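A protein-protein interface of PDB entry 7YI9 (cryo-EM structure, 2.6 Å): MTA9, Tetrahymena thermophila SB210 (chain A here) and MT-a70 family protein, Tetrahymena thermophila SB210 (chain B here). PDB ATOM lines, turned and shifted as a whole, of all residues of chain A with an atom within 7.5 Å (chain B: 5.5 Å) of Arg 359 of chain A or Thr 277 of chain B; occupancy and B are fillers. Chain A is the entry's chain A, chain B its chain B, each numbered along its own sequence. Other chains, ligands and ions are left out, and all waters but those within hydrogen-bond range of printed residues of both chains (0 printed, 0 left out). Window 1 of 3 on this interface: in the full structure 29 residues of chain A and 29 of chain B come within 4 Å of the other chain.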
ATOM      1  N   SER A 188      -6.563   7.780  28.114  1.00  0.00           N
ATOM      2  CA  SER A 188      -6.599   9.084  27.472  1.00  0.00           C
ATOM      3  C   SER A 188      -6.655   8.940  25.960  1.00  0.00           C
ATOM      4  O   SER A 188      -5.972   8.092  25.380  1.00  0.00           O
ATOM      5  CB  SER A 188      -5.381   9.921  27.854  1.00  0.00           C
ATOM      6  OG  SER A 188      -5.564  11.273  27.476  1.00  0.00           O
ATOM      7  N   GLU A 189      -7.475   9.772  25.332  1.00  0.00           N
ATOM      8  CA  GLU A 189      -7.440   9.953  23.892  1.00  0.00           C
ATOM      9  C   GLU A 189      -6.434  11.056  23.571  1.00  0.00           C
ATOM     10  O   GLU A 189      -5.661  11.486  24.429  1.00  0.00           O
ATOM     11  CB  GLU A 189      -8.835  10.272  23.361  1.00  0.00           C
ATOM     12  CG  GLU A 189      -9.743   9.065  23.218  1.00  0.00           C
ATOM     13  CD  GLU A 189      -9.060   7.892  22.546  1.00  0.00           C
ATOM     14  OE1 GLU A 189      -8.991   7.879  21.300  1.00  0.00           O
ATOM     15  OE2 GLU A 189      -8.596   6.979  23.264  1.00  0.00           O
ATOM     16  N   LYS A 190      -6.424  11.523  22.326  1.00  0.00           N
ATOM     17  CA  LYS A 190      -5.567  12.641  21.959  1.00  0.00           C
ATOM     18  C   LYS A 190      -6.275  13.983  22.064  1.00  0.00           C
ATOM     19  O   LYS A 190      -5.604  15.013  22.183  1.00  0.00           O
ATOM     20  CB  LYS A 190      -5.031  12.456  20.535  1.00  0.00           C
ATOM     21  CG  LYS A 190      -3.603  11.935  20.475  1.00  0.00           C
ATOM     22  CD  LYS A 190      -2.914  12.336  19.182  1.00  0.00           C
ATOM     23  CE  LYS A 190      -3.064  11.265  18.117  1.00  0.00           C
ATOM     24  NZ  LYS A 190      -2.237  11.553  16.915  1.00  0.00           N
ATOM     25  N   LEU A 193      -6.526  15.112  26.498  1.00  0.00           N
ATOM     26  CA  LEU A 193      -5.443  14.976  27.469  1.00  0.00           C
ATOM     27  C   LEU A 193      -5.328  16.215  28.351  1.00  0.00           C
ATOM     28  O   LEU A 193      -5.182  16.112  29.577  1.00  0.00           O
ATOM     29  CB  LEU A 193      -4.126  14.699  26.745  1.00  0.00           C
ATOM     30  CG  LEU A 193      -2.953  14.236  27.606  1.00  0.00           C
ATOM     31  CD1 LEU A 193      -2.186  13.149  26.889  1.00  0.00           C
ATOM     32  CD2 LEU A 193      -2.035  15.390  27.941  1.00  0.00           C
ATOM     33  N   ASN A 210       3.119   8.361  32.480  1.00  0.00           N
ATOM     34  CA  ASN A 210       2.365   8.047  31.278  1.00  0.00           C
ATOM     35  C   ASN A 210       2.771   6.653  30.810  1.00  0.00           C
ATOM     36  O   ASN A 210       3.874   6.184  31.101  1.00  0.00           O
ATOM     37  CB  ASN A 210       2.614   9.092  30.183  1.00  0.00           C
ATOM     38  CG  ASN A 210       1.629   8.992  29.043  1.00  0.00           C
ATOM     39  OD1 ASN A 210       0.748   8.135  29.039  1.00  0.00           O
ATOM     40  ND2 ASN A 210       1.771   9.874  28.063  1.00  0.00           N
ATOM     41  N   PHE A 211       1.865   5.993  30.090  1.00  0.00           N
ATOM     42  CA  PHE A 211       2.062   4.627  29.622  1.00  0.00           C
ATOM     43  C   PHE A 211       1.346   4.457  28.292  1.00  0.00           C
ATOM     44  O   PHE A 211       0.137   4.677  28.211  1.00  0.00           O
ATOM     45  CB  PHE A 211       1.535   3.621  30.652  1.00  0.00           C
ATOM     46  CG  PHE A 211       1.609   2.189  30.206  1.00  0.00           C
ATOM     47  CD1 PHE A 211       2.772   1.459  30.372  1.00  0.00           C
ATOM     48  CD2 PHE A 211       0.509   1.568  29.638  1.00  0.00           C
ATOM     49  CE1 PHE A 211       2.842   0.144  29.968  1.00  0.00           C
ATOM     50  CE2 PHE A 211       0.574   0.253  29.234  1.00  0.00           C
ATOM     51  CZ  PHE A 211       1.742  -0.459  29.399  1.00  0.00           C
ATOM     52  N   SER A 212       2.083   4.056  27.257  1.00  0.00           N
ATOM     53  CA  SER A 212       1.541   3.966  25.906  1.00  0.00           C
ATOM     54  C   SER A 212       1.766   2.579  25.320  1.00  0.00           C
ATOM     55  O   SER A 212       2.707   1.871  25.687  1.00  0.00           O
ATOM     56  CB  SER A 212       2.161   5.015  24.977  1.00  0.00           C
ATOM     57  OG  SER A 212       1.663   6.308  25.261  1.00  0.00           O
ATOM     58  N   ILE A 213       0.883   2.204  24.399  1.00  0.00           N
ATOM     59  CA  ILE A 213       0.931   0.925  23.701  1.00  0.00           C
ATOM     60  C   ILE A 213       1.189   1.204  22.228  1.00  0.00           C
ATOM     61  O   ILE A 213       0.388   1.883  21.577  1.00  0.00           O
ATOM     62  CB  ILE A 213      -0.376   0.134  23.869  1.00  0.00           C
ATOM     63  CG1 ILE A 213      -0.751   0.004  25.345  1.00  0.00           C
ATOM     64  CG2 ILE A 213      -0.273  -1.227  23.197  1.00  0.00           C
ATOM     65  CD1 ILE A 213      -2.212  -0.305  25.565  1.00  0.00           C
ATOM     66  N   MET A 214       2.282   0.661  21.694  1.00  0.00           N
ATOM     67  CA  MET A 214       2.564   0.782  20.268  1.00  0.00           C
ATOM     68  C   MET A 214       1.868  -0.338  19.506  1.00  0.00           C
ATOM     69  O   MET A 214       2.033  -1.516  19.831  1.00  0.00           O
ATOM     70  CB  MET A 214       4.069   0.744  20.010  1.00  0.00           C
ATOM     71  CG  MET A 214       4.856   1.773  20.794  1.00  0.00           C
ATOM     72  SD  MET A 214       4.393   3.466  20.393  1.00  0.00           S
ATOM     73  CE  MET A 214       4.654   4.275  21.966  1.00  0.00           C
ATOM     74  N   PHE A 215       1.102   0.028  18.487  1.00  0.00           N
ATOM     75  CA  PHE A 215       0.231  -0.911  17.793  1.00  0.00           C
ATOM     76  C   PHE A 215       0.840  -1.346  16.467  1.00  0.00           C
ATOM     77  O   PHE A 215       1.172  -0.507  15.622  1.00  0.00           O
ATOM     78  CB  PHE A 215      -1.147  -0.292  17.553  1.00  0.00           C
ATOM     79  CG  PHE A 215      -2.026  -0.283  18.770  1.00  0.00           C
ATOM     80  CD1 PHE A 215      -2.042  -1.359  19.638  1.00  0.00           C
ATOM     81  CD2 PHE A 215      -2.839   0.803  19.043  1.00  0.00           C
ATOM     82  CE1 PHE A 215      -2.852  -1.352  20.754  1.00  0.00           C
ATOM     83  CE2 PHE A 215      -3.648   0.813  20.157  1.00  0.00           C
ATOM     84  CZ  PHE A 215      -3.654  -0.265  21.014  1.00  0.00           C
ATOM     85  N   LEU A 348       0.863   0.363  12.749  1.00  0.00           N
ATOM     86  CA  LEU A 348      -0.507   0.738  12.446  1.00  0.00           C
ATOM     87  C   LEU A 348      -0.602   2.242  12.237  1.00  0.00           C
ATOM     88  O   LEU A 348       0.018   3.027  12.957  1.00  0.00           O
ATOM     89  CB  LEU A 348      -1.437   0.297  13.574  1.00  0.00           C
ATOM     90  CG  LEU A 348      -2.935   0.420  13.317  1.00  0.00           C
ATOM     91  CD1 LEU A 348      -3.279  -0.118  11.944  1.00  0.00           C
ATOM     92  CD2 LEU A 348      -3.698  -0.331  14.383  1.00  0.00           C
ATOM     93  N   ASN A 350      -3.657   4.707  11.875  1.00  0.00           N
ATOM     94  CA  ASN A 350      -5.074   5.037  11.871  1.00  0.00           C
ATOM     95  C   ASN A 350      -5.276   6.521  11.592  1.00  0.00           C
ATOM     96  O   ASN A 350      -4.419   7.352  11.897  1.00  0.00           O
ATOM     97  CB  ASN A 350      -5.731   4.665  13.200  1.00  0.00           C
ATOM     98  CG  ASN A 350      -5.960   3.177  13.337  1.00  0.00           C
ATOM     99  OD1 ASN A 350      -5.247   2.492  14.067  1.00  0.00           O
ATOM    100  ND2 ASN A 350      -6.960   2.667  12.631  1.00  0.00           N
ATOM    101  N   PHE A 355      -1.751  13.860  12.942  1.00  0.00           N
ATOM    102  CA  PHE A 355      -0.789  12.801  12.678  1.00  0.00           C
ATOM    103  C   PHE A 355      -1.472  11.458  12.876  1.00  0.00           C
ATOM    104  O   PHE A 355      -2.370  11.332  13.712  1.00  0.00           O
ATOM    105  CB  PHE A 355       0.444  12.898  13.586  1.00  0.00           C
ATOM    106  CG  PHE A 355       1.422  13.959  13.173  1.00  0.00           C
ATOM    107  CD1 PHE A 355       1.282  15.263  13.616  1.00  0.00           C
ATOM    108  CD2 PHE A 355       2.481  13.657  12.335  1.00  0.00           C
ATOM    109  CE1 PHE A 355       2.182  16.241  13.234  1.00  0.00           C
ATOM    110  CE2 PHE A 355       3.383  14.631  11.949  1.00  0.00           C
ATOM    111  CZ  PHE A 355       3.233  15.924  12.399  1.00  0.00           C
ATOM    112  N   LYS A 356      -1.040  10.458  12.115  1.00  0.00           N
ATOM    113  CA  LYS A 356      -1.683   9.151  12.159  1.00  0.00           C
ATOM    114  C   LYS A 356      -1.515   8.505  13.529  1.00  0.00           C
ATOM    115  O   LYS A 356      -0.457   8.599  14.156  1.00  0.00           O
ATOM    116  CB  LYS A 356      -1.109   8.248  11.070  1.00  0.00           C
ATOM    117  CG  LYS A 356      -1.782   8.442   9.732  1.00  0.00           C
ATOM    118  CD  LYS A 356      -1.004   7.813   8.604  1.00  0.00           C
ATOM    119  CE  LYS A 356      -1.806   7.857   7.321  1.00  0.00           C
ATOM    120  NZ  LYS A 356      -3.075   7.094   7.450  1.00  0.00           N
ATOM    121  N   LYS A 357      -2.576   7.845  13.991  1.00  0.00           N
ATOM    122  CA  LYS A 357      -2.594   7.252  15.321  1.00  0.00           C
ATOM    123  C   LYS A 357      -1.887   5.904  15.323  1.00  0.00           C
ATOM    124  O   LYS A 357      -2.182   5.034  14.500  1.00  0.00           O
ATOM    125  CB  LYS A 357      -4.031   7.084  15.811  1.00  0.00           C
ATOM    126  CG  LYS A 357      -4.748   8.383  16.092  1.00  0.00           C
ATOM    127  CD  LYS A 357      -6.191   8.139  16.475  1.00  0.00           C
ATOM    128  CE  LYS A 357      -6.289   7.543  17.864  1.00  0.00           C
ATOM    129  NZ  LYS A 357      -7.698   7.458  18.328  1.00  0.00           N
ATOM    130  N   THR A 358      -0.966   5.730  16.263  1.00  0.00           N
ATOM    131  CA  THR A 358      -0.234   4.481  16.403  1.00  0.00           C
ATOM    132  C   THR A 358      -0.138   4.006  17.847  1.00  0.00           C
ATOM    133  O   THR A 358       0.409   2.926  18.083  1.00  0.00           O
ATOM    134  CB  THR A 358       1.181   4.637  15.812  1.00  0.00           C
ATOM    135  OG1 THR A 358       1.101   5.358  14.579  1.00  0.00           O
ATOM    136  CG2 THR A 358       1.828   3.288  15.525  1.00  0.00           C
ATOM    137  N   ARG A 359      -0.666   4.748  18.818  1.00  0.00           N
ATOM    138  CA  ARG A 359      -0.508   4.399  20.221  1.00  0.00           C
ATOM    139  C   ARG A 359      -1.802   4.659  20.982  1.00  0.00           C
ATOM    140  O   ARG A 359      -2.715   5.330  20.501  1.00  0.00           O
ATOM    141  CB  ARG A 359       0.646   5.174  20.866  1.00  0.00           C
ATOM    142  CG  ARG A 359       0.328   6.629  21.069  1.00  0.00           C
ATOM    143  CD  ARG A 359       1.409   7.366  21.821  1.00  0.00           C
ATOM    144  NE  ARG A 359       0.981   8.730  22.093  1.00  0.00           N
ATOM    145  CZ  ARG A 359       1.109   9.738  21.240  1.00  0.00           C
ATOM    146  NH1 ARG A 359       1.716   9.585  20.078  1.00  0.00           N
ATOM    147  NH2 ARG A 359       0.614  10.927  21.562  1.00  0.00           N
ATOM    148  N   HIS A 360      -1.868   4.092  22.185  1.00  0.00           N
ATOM    149  CA  HIS A 360      -2.947   4.317  23.137  1.00  0.00           C
ATOM    150  C   HIS A 360      -2.324   4.517  24.509  1.00  0.00           C
ATOM    151  O   HIS A 360      -1.514   3.696  24.944  1.00  0.00           O
ATOM    152  CB  HIS A 360      -3.925   3.140  23.162  1.00  0.00           C
ATOM    153  CG  HIS A 360      -5.169   3.403  23.949  1.00  0.00           C
ATOM    154  ND1 HIS A 360      -5.450   2.762  25.135  1.00  0.00           N
ATOM    155  CD2 HIS A 360      -6.209   4.238  23.717  1.00  0.00           C
ATOM    156  CE1 HIS A 360      -6.608   3.192  25.601  1.00  0.00           C
ATOM    157  NE2 HIS A 360      -7.089   4.088  24.760  1.00  0.00           N
ATOM    158  N   THR A 361      -2.704   5.593  25.192  1.00  0.00           N
ATOM    159  CA  THR A 361      -1.987   6.033  26.380  1.00  0.00           C
ATOM    160  C   THR A 361      -2.865   5.973  27.624  1.00  0.00           C
ATOM    161  O   THR A 361      -4.084   6.145  27.561  1.00  0.00           O
ATOM    162  CB  THR A 361      -1.434   7.455  26.190  1.00  0.00           C
ATOM    163  OG1 THR A 361      -0.693   7.844  27.352  1.00  0.00           O
ATOM    164  CG2 THR A 361      -2.556   8.450  25.943  1.00  0.00           C
ATOM    165  N   VAL A 385       6.494   1.802  27.302  1.00  0.00           N
ATOM    166  CA  VAL A 385       6.165   1.407  25.939  1.00  0.00           C
ATOM    167  C   VAL A 385       5.976  -0.102  25.907  1.00  0.00           C
ATOM    168  O   VAL A 385       6.818  -0.848  26.420  1.00  0.00           O
ATOM    169  CB  VAL A 385       7.260   1.842  24.948  1.00  0.00           C
ATOM    170  CG1 VAL A 385       6.989   1.278  23.570  1.00  0.00           C
ATOM    171  CG2 VAL A 385       7.360   3.354  24.898  1.00  0.00           C
ATOM    172  N   VAL A 386       4.871  -0.545  25.318  1.00  0.00           N
ATOM    173  CA  VAL A 386       4.635  -1.956  25.055  1.00  0.00           C
ATOM    174  C   VAL A 386       4.146  -2.087  23.620  1.00  0.00           C
ATOM    175  O   VAL A 386       3.454  -1.209  23.095  1.00  0.00           O
ATOM    176  CB  VAL A 386       3.630  -2.581  26.055  1.00  0.00           C
ATOM    177  CG1 VAL A 386       2.219  -2.066  25.815  1.00  0.00           C
ATOM    178  CG2 VAL A 386       3.678  -4.099  25.997  1.00  0.00           C
ATOM    179  N   PRO A 395      -8.862  -0.282  18.092  1.00  0.00           N
ATOM    180  CA  PRO A 395      -7.769  -0.624  19.014  1.00  0.00           C
ATOM    181  C   PRO A 395      -7.903  -0.004  20.394  1.00  0.00           C
ATOM    182  O   PRO A 395      -7.208  -0.446  21.316  1.00  0.00           O
ATOM    183  CB  PRO A 395      -6.524  -0.100  18.287  1.00  0.00           C
ATOM    184  CG  PRO A 395      -7.038   0.976  17.406  1.00  0.00           C
ATOM    185  CD  PRO A 395      -8.391   0.524  16.956  1.00  0.00           C
ATOM    186  N   SER A 396      -8.757   1.008  20.566  1.00  0.00           N
ATOM    187  CA  SER A 396      -8.940   1.605  21.885  1.00  0.00           C
ATOM    188  C   SER A 396      -9.520   0.597  22.869  1.00  0.00           C
ATOM    189  O   SER A 396      -9.154   0.589  24.050  1.00  0.00           O
ATOM    190  CB  SER A 396      -9.841   2.834  21.787  1.00  0.00           C
ATOM    191  OG  SER A 396      -9.316   3.774  20.869  1.00  0.00           O
ATOM    192  N   ASP B 274      -2.249  17.507  19.681  1.00  0.00           N
ATOM    193  CA  ASP B 274      -1.513  16.338  19.228  1.00  0.00           C
ATOM    194  C   ASP B 274      -0.255  16.190  20.064  1.00  0.00           C
ATOM    195  O   ASP B 274       0.084  17.058  20.870  1.00  0.00           O
ATOM    196  CB  ASP B 274      -1.165  16.443  17.739  1.00  0.00           C
ATOM    197  CG  ASP B 274      -0.935  15.091  17.093  1.00  0.00           C
ATOM    198  OD1 ASP B 274      -0.309  14.218  17.729  1.00  0.00           O
ATOM    199  OD2 ASP B 274      -1.386  14.901  15.948  1.00  0.00           O
ATOM    200  N   GLU B 275       0.427  15.070  19.860  1.00  0.00           N
ATOM    201  CA  GLU B 275       1.637  14.758  20.600  1.00  0.00           C
ATOM    202  C   GLU B 275       2.344  13.613  19.891  1.00  0.00           C
ATOM    203  O   GLU B 275       1.750  12.560  19.650  1.00  0.00           O
ATOM    204  CB  GLU B 275       1.304  14.405  22.054  1.00  0.00           C
ATOM    205  CG  GLU B 275       2.488  14.303  22.981  1.00  0.00           C
ATOM    206  CD  GLU B 275       3.062  12.912  23.033  1.00  0.00           C
ATOM    207  OE1 GLU B 275       2.293  11.951  22.848  1.00  0.00           O
ATOM    208  OE2 GLU B 275       4.279  12.774  23.256  1.00  0.00           O
ATOM    209  N   ILE B 276       3.610  13.833  19.550  1.00  0.00           N
ATOM    210  CA  ILE B 276       4.420  12.859  18.829  1.00  0.00           C
ATOM    211  C   ILE B 276       5.375  12.214  19.817  1.00  0.00           C
ATOM    212  O   ILE B 276       6.113  12.907  20.523  1.00  0.00           O
ATOM    213  CB  ILE B 276       5.187  13.503  17.660  1.00  0.00           C
ATOM    214  CG1 ILE B 276       4.260  13.735  16.471  1.00  0.00           C
ATOM    215  CG2 ILE B 276       6.345  12.627  17.226  1.00  0.00           C
ATOM    216  CD1 ILE B 276       4.926  14.447  15.322  1.00  0.00           C
ATOM    217  N   THR B 277       5.362  10.888  19.862  1.00  0.00           N
ATOM    218  CA  THR B 277       6.239  10.121  20.731  1.00  0.00           C
ATOM    219  C   THR B 277       7.418   9.595  19.925  1.00  0.00           C
ATOM    220  O   THR B 277       7.231   8.971  18.878  1.00  0.00           O
ATOM    221  CB  THR B 277       5.479   8.962  21.379  1.00  0.00           C
ATOM    222  OG1 THR B 277       4.626   9.466  22.414  1.00  0.00           O
ATOM    223  CG2 THR B 277       6.439   7.955  21.966  1.00  0.00           C
ATOM    224  N   TRP B 278       8.625   9.859  20.402  1.00  0.00           N
ATOM    225  CA  TRP B 278       9.836   9.323  19.797  1.00  0.00           C
ATOM    226  C   TRP B 278      10.315   8.171  20.671  1.00  0.00           C
ATOM    227  O   TRP B 278      10.784   8.388  21.792  1.00  0.00           O
ATOM    228  CB  TRP B 278      10.903  10.407  19.649  1.00  0.00           C
ATOM    229  CG  TRP B 278      12.272   9.882  19.328  1.00  0.00           C
ATOM    230  CD1 TRP B 278      12.579   8.829  18.518  1.00  0.00           C
ATOM    231  CD2 TRP B 278      13.518  10.391  19.810  1.00  0.00           C
ATOM    232  NE1 TRP B 278      13.935   8.647  18.472  1.00  0.00           N
ATOM    233  CE2 TRP B 278      14.536   9.596  19.255  1.00  0.00           C
ATOM    234  CE3 TRP B 278      13.871  11.446  20.656  1.00  0.00           C
ATOM    235  CZ2 TRP B 278      15.883   9.819  19.518  1.00  0.00           C
ATOM    236  CZ3 TRP B 278      15.206  11.666  20.916  1.00  0.00           C
ATOM    237  CH2 TRP B 278      16.198  10.856  20.350  1.00  0.00           C
ATOM    238  N   VAL B 279      10.188   6.952  20.160  1.00  0.00           N
ATOM    239  CA  VAL B 279      10.651   5.759  20.858  1.00  0.00           C
ATOM    240  C   VAL B 279      12.075   5.468  20.411  1.00  0.00           C
ATOM    241  O   VAL B 279      12.346   5.340  19.213  1.00  0.00           O
ATOM    242  CB  VAL B 279       9.725   4.564  20.580  1.00  0.00           C
ATOM    243  CG1 VAL B 279      10.076   3.398  21.483  1.00  0.00           C
ATOM    244  CG2 VAL B 279       8.273   4.964  20.762  1.00  0.00           C
ATOM    245  N   LYS B 299      10.766   6.871  25.966  1.00  0.00           N
ATOM    246  CA  LYS B 299      10.229   7.732  24.926  1.00  0.00           C
ATOM    247  C   LYS B 299      10.355   9.183  25.360  1.00  0.00           C
ATOM    248  O   LYS B 299      10.554   9.486  26.538  1.00  0.00           O
ATOM    249  CB  LYS B 299       8.767   7.393  24.617  1.00  0.00           C
ATOM    250  CG  LYS B 299       7.885   7.236  25.843  1.00  0.00           C
ATOM    251  CD  LYS B 299       6.415   7.344  25.475  1.00  0.00           C
ATOM    252  CE  LYS B 299       5.513   6.848  26.590  1.00  0.00           C
ATOM    253  NZ  LYS B 299       5.925   7.384  27.912  1.00  0.00           N
ATOM    254  N   GLU B 300      10.245  10.081  24.384  1.00  0.00           N
ATOM    255  CA  GLU B 300      10.179  11.512  24.629  1.00  0.00           C
ATOM    256  C   GLU B 300       8.976  12.096  23.910  1.00  0.00           C
ATOM    257  O   GLU B 300       8.542  11.590  22.875  1.00  0.00           O
ATOM    258  CB  GLU B 300      11.447  12.245  24.187  1.00  0.00           C
ATOM    259  CG  GLU B 300      12.669  11.901  25.003  1.00  0.00           C
ATOM    260  CD  GLU B 300      13.905  12.628  24.528  1.00  0.00           C
ATOM    261  OE1 GLU B 300      13.828  13.302  23.481  1.00  0.00           O
ATOM    262  OE2 GLU B 300      14.952  12.532  25.199  1.00  0.00           O
ATOM    263  N   SER B 301       8.454  13.181  24.469  1.00  0.00           N
ATOM    264  CA  SER B 301       7.193  13.769  24.048  1.00  0.00           C
ATOM    265  C   SER B 301       7.435  15.099  23.351  1.00  0.00           C
ATOM    266  O   SER B 301       8.205  15.931  23.838  1.00  0.00           O
ATOM    267  CB  SER B 301       6.276  13.970  25.255  1.00  0.00           C
ATOM    268  OG  SER B 301       5.012  14.461  24.855  1.00  0.00           O
ATOM    269  N   CYS B 302       6.777  15.296  22.216  1.00  0.00           N
ATOM    270  CA  CYS B 302       6.767  16.573  21.513  1.00  0.00           C
ATOM    271  C   CYS B 302       5.318  17.049  21.475  1.00  0.00           C
ATOM    272  O   CYS B 302       4.554  16.683  20.582  1.00  0.00           O
ATOM    273  CB  CYS B 302       7.355  16.447  20.109  1.00  0.00           C
ATOM    274  SG  CYS B 302       7.458  18.005  19.202  1.00  0.00           S
ATOM    275  N   ASP B 322       2.342   9.222  14.691  1.00  0.00           N
ATOM    276  CA  ASP B 322       2.721   9.940  15.895  1.00  0.00           C
ATOM    277  C   ASP B 322       3.807   9.221  16.682  1.00  0.00           C
ATOM    278  O   ASP B 322       4.047   9.562  17.843  1.00  0.00           O
ATOM    279  CB  ASP B 322       1.485  10.180  16.770  1.00  0.00           C
ATOM    280  CG  ASP B 322       0.841   8.889  17.256  1.00  0.00           C
ATOM    281  OD1 ASP B 322       1.312   7.793  16.892  1.00  0.00           O
ATOM    282  OD2 ASP B 322      -0.149   8.968  18.010  1.00  0.00           O
ATOM    283  N   VAL B 323       4.455   8.231  16.077  1.00  0.00           N
ATOM    284  CA  VAL B 323       5.534   7.477  16.701  1.00  0.00           C
ATOM    285  C   VAL B 323       6.749   7.543  15.788  1.00  0.00           C
ATOM    286  O   VAL B 323       6.631   7.334  14.575  1.00  0.00           O
ATOM    287  CB  VAL B 323       5.127   6.017  16.970  1.00  0.00           C
ATOM    288  CG1 VAL B 323       6.259   5.257  17.631  1.00  0.00           C
ATOM    289  CG2 VAL B 323       3.886   5.969  17.833  1.00  0.00           C
ATOM    290  N   ILE B 324       7.905   7.851  16.364  1.00  0.00           N
ATOM    291  CA  ILE B 324       9.184   7.783  15.670  1.00  0.00           C
ATOM    292  C   ILE B 324      10.008   6.714  16.366  1.00  0.00           C
ATOM    293  O   ILE B 324      10.335   6.844  17.551  1.00  0.00           O
ATOM    294  CB  ILE B 324       9.916   9.131  15.669  1.00  0.00           C
ATOM    295  CG1 ILE B 324       9.138  10.163  14.856  1.00  0.00           C
ATOM    296  CG2 ILE B 324      11.322   8.971  15.116  1.00  0.00           C
ATOM    297  CD1 ILE B 324       9.731  11.547  14.906  1.00  0.00           C
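NZ of Lys 190 of chain A is in salt-bridge range of OD1 of Asp 274 of chain B (3.4 Å).
The side-chain carboxylate (OD2) of Asp 322 of chain B is in salt-bridge range of the side-chain amino group (NZ) of Lys 190 of chain A, at 3.5 Å.
The backbone NH (N) of Phe 355 of chain A sits at hydrogen-bond distance from the side-chain carboxylate (OD2) of Asp 274 of chain B.
N of Asp 322 of chain B lies within hydrogen-bond range of O of Lys 356 of chain A (2.9 Å).
The backbone NH (N) of Thr 358 of chain A lies within hydrogen-bond range of the side-chain carboxylate (OD1) of Asp 322 of chain B (3.1 Å).
NE of Arg 359 of chain A is in salt-bridge range of OE1 of Glu 275 of chain B, 3.6 Å away.
NH1 of Arg 359 of chain A is in salt-bridge range of OD2 of Asp 322 of chain B (2.9 Å).
The side-chain amino group (NZ) of Lys 190 of chain A sits at hydrogen-bond distance from the backbone carbonyl oxygen (O) of Phe 355 of chain A, 3.2 Å away.
The backbone NH of Met 214 of chain A lies within hydrogen-bond range of the backbone carbonyl oxygen of Val 386 of chain A (2.6 Å).
O of Leu 348 of chain A sits at hydrogen-bond distance from OG1 of Thr 358 of chain A (3.0 Å).
OE2 of Glu 275 of chain B is in hydrogen-bond range of OG of Ser 301 of chain B, at 2.4 Å.
The backbone NH of Thr 277 of chain B lies within hydrogen-bond range of the backbone carbonyl oxygen of Asp 322 of chain B (2.8 Å).
O of Ile 324 of chain B lies within hydrogen-bond range of N of Val 279 of chain B (2.6 Å).
Among the printed residues, merely in contact across the chains: Met 214 of chain A with Val 323 of chain B, Thr 358 of chain A with Val 323 of chain B, Phe 355 of chain A with Ile 276 of chain B, Arg 359 of chain A with Thr 277 of chain B, Met 214 of chain A with Val 279 of chain B and Asn 210 of chain A with Lys 299 of chain B.
Printed residues of chain B within 4 Å of Lys 190 of chain A: Asp 274 (3.4 Å) and Asp 322 (3.5 Å).
Ile 213 of chain A touches none of the printed residues of chain B.
Of the printed residues of chain B, Met 214 of chain A touches Val 279 and Val 323.
Printed residues of chain B within 4 Å of Phe 355 of chain A: Asp 274 and Ile 276.
Printed residues of chain B within 4 Å of Arg 359 of chain A: Glu 275 (2.3 Å), Thr 277 (3.7 Å) and Asp 322 (2.9 Å).
Of the printed residues of chain A, Asp 274 of chain B touches Lys 190 and Phe 355.
Trp 278 of chain B touches none of the printed residues of chain A.
Of the printed residues of chain A, Asp 322 of chain B touches Lys 190, Lys 356, Thr 358 and Arg 359.
The nearest residue of chain B that does not touch Arg 359 of chain A is Ile 276 of chain B (4.4 Å).
Of the 23 printed residues of chain A, 7 touch a printed residue of chain B.
Hydrophobic or aromatic side chains of chain A that line the printed part of chain B: Met 214 and Phe 355.
Hydrophobic or aromatic side chains of chain B that line the printed part of chain A: Ile 276, Val 279 and Val 323.
Among the printed residues, Asp or Glu carboxylates within 4 Å of a Lys or Arg side-chain nitrogen of the other chain: Lys 190 of chain A with Asp 274 of chain B (3.4 Å), Lys 190 of chain A with Asp 322 of chain B (3.5 Å), Arg 359 of chain A with Glu 275 of chain B (2.3 Å) and Arg 359 of chain A with Asp 322 of chain B (2.9 Å).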
